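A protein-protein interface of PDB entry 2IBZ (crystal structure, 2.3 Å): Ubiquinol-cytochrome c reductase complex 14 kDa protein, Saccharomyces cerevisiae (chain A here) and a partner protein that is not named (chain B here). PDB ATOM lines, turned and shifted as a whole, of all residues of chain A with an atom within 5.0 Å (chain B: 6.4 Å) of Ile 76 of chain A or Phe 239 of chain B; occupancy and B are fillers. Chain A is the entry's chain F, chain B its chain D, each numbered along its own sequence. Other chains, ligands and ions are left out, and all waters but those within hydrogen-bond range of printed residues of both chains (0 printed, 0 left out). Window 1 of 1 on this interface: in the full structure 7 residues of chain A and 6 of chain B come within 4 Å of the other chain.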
ATOM      1  N   ARG A  71     -15.889   6.627  14.302  1.00  0.00           N
ATOM      2  CA  ARG A  71     -16.630   7.786  13.815  1.00  0.00           C
ATOM      3  C   ARG A  71     -16.159   8.096  12.385  1.00  0.00           C
ATOM      4  O   ARG A  71     -16.979   8.320  11.489  1.00  0.00           O
ATOM      5  CB  ARG A  71     -16.413   9.022  14.720  1.00  0.00           C
ATOM      6  CG  ARG A  71     -17.419  10.141  14.444  1.00  0.00           C
ATOM      7  CD  ARG A  71     -17.150  11.449  15.186  1.00  0.00           C
ATOM      8  NE  ARG A  71     -15.978  12.039  14.591  1.00  0.00           N
ATOM      9  CZ  ARG A  71     -15.893  13.235  14.036  1.00  0.00           C
ATOM     10  NH1 ARG A  71     -14.731  13.561  13.515  1.00  0.00           N
ATOM     11  NH2 ARG A  71     -16.897  14.119  14.058  1.00  0.00           N
ATOM     12  N   ALA A  72     -14.845   8.023  12.169  1.00  0.00           N
ATOM     13  CA  ALA A  72     -14.248   8.305  10.859  1.00  0.00           C
ATOM     14  C   ALA A  72     -14.791   7.381   9.773  1.00  0.00           C
ATOM     15  O   ALA A  72     -15.150   7.831   8.677  1.00  0.00           O
ATOM     16  CB  ALA A  72     -12.723   8.202  10.933  1.00  0.00           C
ATOM     17  N   TYR A  73     -14.853   6.090  10.079  1.00  0.00           N
ATOM     18  CA  TYR A  73     -15.377   5.121   9.125  1.00  0.00           C
ATOM     19  C   TYR A  73     -16.859   5.359   8.841  1.00  0.00           C
ATOM     20  O   TYR A  73     -17.291   5.281   7.689  1.00  0.00           O
ATOM     21  CB  TYR A  73     -15.175   3.681   9.630  1.00  0.00           C
ATOM     22  CG  TYR A  73     -15.791   2.654   8.718  1.00  0.00           C
ATOM     23  CD1 TYR A  73     -15.361   2.527   7.399  1.00  0.00           C
ATOM     24  CD2 TYR A  73     -16.859   1.860   9.143  1.00  0.00           C
ATOM     25  CE1 TYR A  73     -15.981   1.639   6.520  1.00  0.00           C
ATOM     26  CE2 TYR A  73     -17.489   0.967   8.268  1.00  0.00           C
ATOM     27  CZ  TYR A  73     -17.045   0.865   6.959  1.00  0.00           C
ATOM     28  OH  TYR A  73     -17.660  -0.003   6.076  1.00  0.00           O
ATOM     29  N   ARG A  74     -17.636   5.633   9.886  1.00  0.00           N
ATOM     30  CA  ARG A  74     -19.070   5.860   9.716  1.00  0.00           C
ATOM     31  C   ARG A  74     -19.351   7.074   8.840  1.00  0.00           C
ATOM     32  O   ARG A  74     -20.218   7.029   7.957  1.00  0.00           O
ATOM     33  CB  ARG A  74     -19.783   5.988  11.068  1.00  0.00           C
ATOM     34  CG  ARG A  74     -19.846   4.694  11.866  1.00  0.00           C
ATOM     35  CD  ARG A  74     -20.874   4.781  12.991  1.00  0.00           C
ATOM     36  NE  ARG A  74     -20.588   5.864  13.936  1.00  0.00           N
ATOM     37  CZ  ARG A  74     -19.772   5.763  14.978  1.00  0.00           C
ATOM     38  NH1 ARG A  74     -19.574   6.810  15.769  1.00  0.00           N
ATOM     39  NH2 ARG A  74     -19.161   4.618  15.234  1.00  0.00           N
ATOM     40  N   ILE A  75     -18.586   8.140   9.062  1.00  0.00           N
ATOM     41  CA  ILE A  75     -18.723   9.368   8.284  1.00  0.00           C
ATOM     42  C   ILE A  75     -18.344   9.146   6.806  1.00  0.00           C
ATOM     43  O   ILE A  75     -19.087   9.534   5.883  1.00  0.00           O
ATOM     44  CB  ILE A  75     -17.896  10.501   8.921  1.00  0.00           C
ATOM     45  CG1 ILE A  75     -18.556  10.918  10.245  1.00  0.00           C
ATOM     46  CG2 ILE A  75     -17.781  11.698   7.963  1.00  0.00           C
ATOM     47  CD1 ILE A  75     -17.729  11.871  11.086  1.00  0.00           C
ATOM     48  N   ILE A  76     -17.225   8.468   6.577  1.00  0.00           N
ATOM     49  CA  ILE A  76     -16.800   8.199   5.207  1.00  0.00           C
ATOM     50  C   ILE A  76     -17.814   7.313   4.500  1.00  0.00           C
ATOM     51  O   ILE A  76     -18.218   7.591   3.367  1.00  0.00           O
ATOM     52  CB  ILE A  76     -15.396   7.567   5.146  1.00  0.00           C
ATOM     53  CG1 ILE A  76     -14.360   8.569   5.655  1.00  0.00           C
ATOM     54  CG2 ILE A  76     -15.056   7.167   3.726  1.00  0.00           C
ATOM     55  CD1 ILE A  76     -12.969   8.002   5.783  1.00  0.00           C
ATOM     56  N   ARG A  77     -18.274   6.281   5.192  1.00  0.00           N
ATOM     57  CA  ARG A  77     -19.264   5.353   4.627  1.00  0.00           C
ATOM     58  C   ARG A  77     -20.581   6.080   4.288  1.00  0.00           C
ATOM     59  O   ARG A  77     -21.213   5.804   3.267  1.00  0.00           O
ATOM     60  CB  ARG A  77     -19.492   4.187   5.601  1.00  0.00           C
ATOM     61  CG  ARG A  77     -20.452   3.120   5.141  1.00  0.00           C
ATOM     62  CD  ARG A  77     -21.443   2.846   6.258  1.00  0.00           C
ATOM     63  NE  ARG A  77     -21.137   1.655   7.045  1.00  0.00           N
ATOM     64  CZ  ARG A  77     -21.359   1.518   8.349  1.00  0.00           C
ATOM     65  NH1 ARG A  77     -21.053   0.370   8.933  1.00  0.00           N
ATOM     66  NH2 ARG A  77     -21.825   2.525   9.080  1.00  0.00           N
ATOM     67  N   ALA A  78     -20.966   7.040   5.126  1.00  0.00           N
ATOM     68  CA  ALA A  78     -22.183   7.815   4.875  1.00  0.00           C
ATOM     69  C   ALA A  78     -22.046   8.689   3.607  1.00  0.00           C
ATOM     70  O   ALA A  78     -22.986   8.771   2.801  1.00  0.00           O
ATOM     71  CB  ALA A  78     -22.531   8.676   6.096  1.00  0.00           C
ATOM     72  N   HIS A  79     -20.887   9.334   3.420  1.00  0.00           N
ATOM     73  CA  HIS A  79     -20.684  10.163   2.227  1.00  0.00           C
ATOM     74  C   HIS A  79     -20.732   9.347   0.948  1.00  0.00           C
ATOM     75  O   HIS A  79     -21.365   9.763  -0.032  1.00  0.00           O
ATOM     76  CB  HIS A  79     -19.373  10.952   2.293  1.00  0.00           C
ATOM     77  CG  HIS A  79     -19.454  12.180   3.146  1.00  0.00           C
ATOM     78  ND1 HIS A  79     -18.778  12.306   4.341  1.00  0.00           N
ATOM     79  CD2 HIS A  79     -20.123  13.342   2.967  1.00  0.00           C
ATOM     80  CE1 HIS A  79     -19.023  13.495   4.860  1.00  0.00           C
ATOM     81  NE2 HIS A  79     -19.837  14.145   4.044  1.00  0.00           N
ATOM     82  N   GLN A  80     -20.075   8.187   0.964  1.00  0.00           N
ATOM     83  CA  GLN A  80     -20.052   7.302  -0.195  1.00  0.00           C
ATOM     84  C   GLN A  80     -21.450   6.795  -0.542  1.00  0.00           C
ATOM     85  O   GLN A  80     -21.831   6.757  -1.715  1.00  0.00           O
ATOM     86  CB  GLN A  80     -19.127   6.114   0.047  1.00  0.00           C
ATOM     87  CG  GLN A  80     -19.111   5.133  -1.108  1.00  0.00           C
ATOM     88  CD  GLN A  80     -18.529   5.730  -2.380  1.00  0.00           C
ATOM     89  OE1 GLN A  80     -17.662   6.607  -2.332  1.00  0.00           O
ATOM     90  NE2 GLN A  80     -19.000   5.255  -3.524  1.00  0.00           N
ATOM     91  N   ARG B 237     -16.656   2.819  -5.953  1.00  0.00           N
ATOM     92  CA  ARG B 237     -15.616   2.678  -4.942  1.00  0.00           C
ATOM     93  C   ARG B 237     -16.192   1.919  -3.739  1.00  0.00           C
ATOM     94  O   ARG B 237     -17.371   2.073  -3.421  1.00  0.00           O
ATOM     95  CB  ARG B 237     -15.171   4.090  -4.542  1.00  0.00           C
ATOM     96  CG  ARG B 237     -14.042   4.207  -3.553  1.00  0.00           C
ATOM     97  CD  ARG B 237     -13.590   5.672  -3.477  1.00  0.00           C
ATOM     98  NE  ARG B 237     -14.695   6.583  -3.176  1.00  0.00           N
ATOM     99  CZ  ARG B 237     -14.564   7.740  -2.527  1.00  0.00           C
ATOM    100  NH1 ARG B 237     -15.633   8.490  -2.286  1.00  0.00           N
ATOM    101  NH2 ARG B 237     -13.365   8.164  -2.139  1.00  0.00           N
ATOM    102  N   LYS B 238     -15.376   1.075  -3.104  1.00  0.00           N
ATOM    103  CA  LYS B 238     -15.817   0.298  -1.942  1.00  0.00           C
ATOM    104  C   LYS B 238     -14.875   0.412  -0.757  1.00  0.00           C
ATOM    105  O   LYS B 238     -13.656   0.407  -0.917  1.00  0.00           O
ATOM    106  CB  LYS B 238     -16.002  -1.175  -2.313  1.00  0.00           C
ATOM    107  CG  LYS B 238     -17.002  -1.372  -3.433  1.00  0.00           C
ATOM    108  CD  LYS B 238     -17.565  -2.769  -3.490  1.00  0.00           C
ATOM    109  CE  LYS B 238     -18.631  -2.856  -4.575  1.00  0.00           C
ATOM    110  NZ  LYS B 238     -19.332  -4.182  -4.587  1.00  0.00           N
ATOM    111  N   PHE B 239     -15.450   0.510   0.436  1.00  0.00           N
ATOM    112  CA  PHE B 239     -14.669   0.630   1.668  1.00  0.00           C
ATOM    113  C   PHE B 239     -14.811  -0.596   2.605  1.00  0.00           C
ATOM    114  O   PHE B 239     -15.809  -1.332   2.554  1.00  0.00           O
ATOM    115  CB  PHE B 239     -15.095   1.892   2.442  1.00  0.00           C
ATOM    116  CG  PHE B 239     -14.722   3.187   1.773  1.00  0.00           C
ATOM    117  CD1 PHE B 239     -15.534   3.738   0.781  1.00  0.00           C
ATOM    118  CD2 PHE B 239     -13.561   3.865   2.136  1.00  0.00           C
ATOM    119  CE1 PHE B 239     -15.194   4.945   0.155  1.00  0.00           C
ATOM    120  CE2 PHE B 239     -13.208   5.071   1.517  1.00  0.00           C
ATOM    121  CZ  PHE B 239     -14.031   5.610   0.523  1.00  0.00           C
ATOM    122  N   VAL B 240     -13.783  -0.827   3.424  1.00  0.00           N
ATOM    123  CA  VAL B 240     -13.785  -1.900   4.419  1.00  0.00           C
ATOM    124  C   VAL B 240     -13.097  -1.397   5.687  1.00  0.00           C
ATOM    125  O   VAL B 240     -12.052  -0.762   5.635  1.00  0.00           O
ATOM    126  CB  VAL B 240     -13.072  -3.191   3.948  1.00  0.00           C
ATOM    127  CG1 VAL B 240     -13.811  -3.814   2.797  1.00  0.00           C
ATOM    128  CG2 VAL B 240     -11.632  -2.906   3.582  1.00  0.00           C
ATOM    129  N   PHE B 241     -13.696  -1.679   6.831  1.00  0.00           N
ATOM    130  CA  PHE B 241     -13.125  -1.246   8.095  1.00  0.00           C
ATOM    131  C   PHE B 241     -12.687  -2.449   8.945  1.00  0.00           C
ATOM    132  O   PHE B 241     -13.422  -3.428   9.089  1.00  0.00           O
ATOM    133  CB  PHE B 241     -14.161  -0.407   8.842  1.00  0.00           C
ATOM    134  CG  PHE B 241     -13.689   0.134  10.164  1.00  0.00           C
ATOM    135  CD1 PHE B 241     -12.478   0.827  10.271  1.00  0.00           C
ATOM    136  CD2 PHE B 241     -14.481  -0.002  11.298  1.00  0.00           C
ATOM    137  CE1 PHE B 241     -12.065   1.383  11.486  1.00  0.00           C
ATOM    138  CE2 PHE B 241     -14.077   0.549  12.521  1.00  0.00           C
ATOM    139  CZ  PHE B 241     -12.864   1.245  12.613  1.00  0.00           C
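OE1 of Gln 80 of chain A sits at hydrogen-bond distance from NH1 of Arg 237 of chain B (2.8 Å).
Phe 241 of chain B touches Tyr 73 of chain A (CB to CG, 3.5 Å).
Phe 239 of chain B touches Ile 76 of chain A.
Gln 80 of chain A touches Phe 239 of chain B.
Phe 239 of chain B touches just these residues of chain A: Ile 76 (3.6 Å) and Gln 80 (3.9 Å).
Printed residues of chain A within 4 Å of Arg 237 of chain B: Gln 80 (2.8 Å).
Of the printed residues of chain B, Tyr 73 of chain A touches Phe 241 (3.5 Å).
Of the printed residues of chain B, Gln 80 of chain A touches Arg 237 and Phe 239.
Of the printed residues of chain A, Phe 241 of chain B touches Tyr 73.
The nearest residue of chain B that does not touch Ile 76 of chain A is Arg 237 of chain B (6.2 Å).
The nearest residue of chain A that does not touch Phe 239 of chain B is Tyr 73 of chain A (4.2 Å).
The nearest printed residue of chain A that does not touch Arg 237 of chain B is His 79 of chain A (6.1 Å).
Of the 5 printed residues of chain B, 3 touch a printed residue of chain A.
Hydrophobic or aromatic side chains of chain A that line the printed part of chain B: Tyr 73 and Ile 76.
Among the printed residues, no Asp or Glu carboxylate lies within 4 Å of a Lys or Arg side-chain nitrogen of the other chain.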
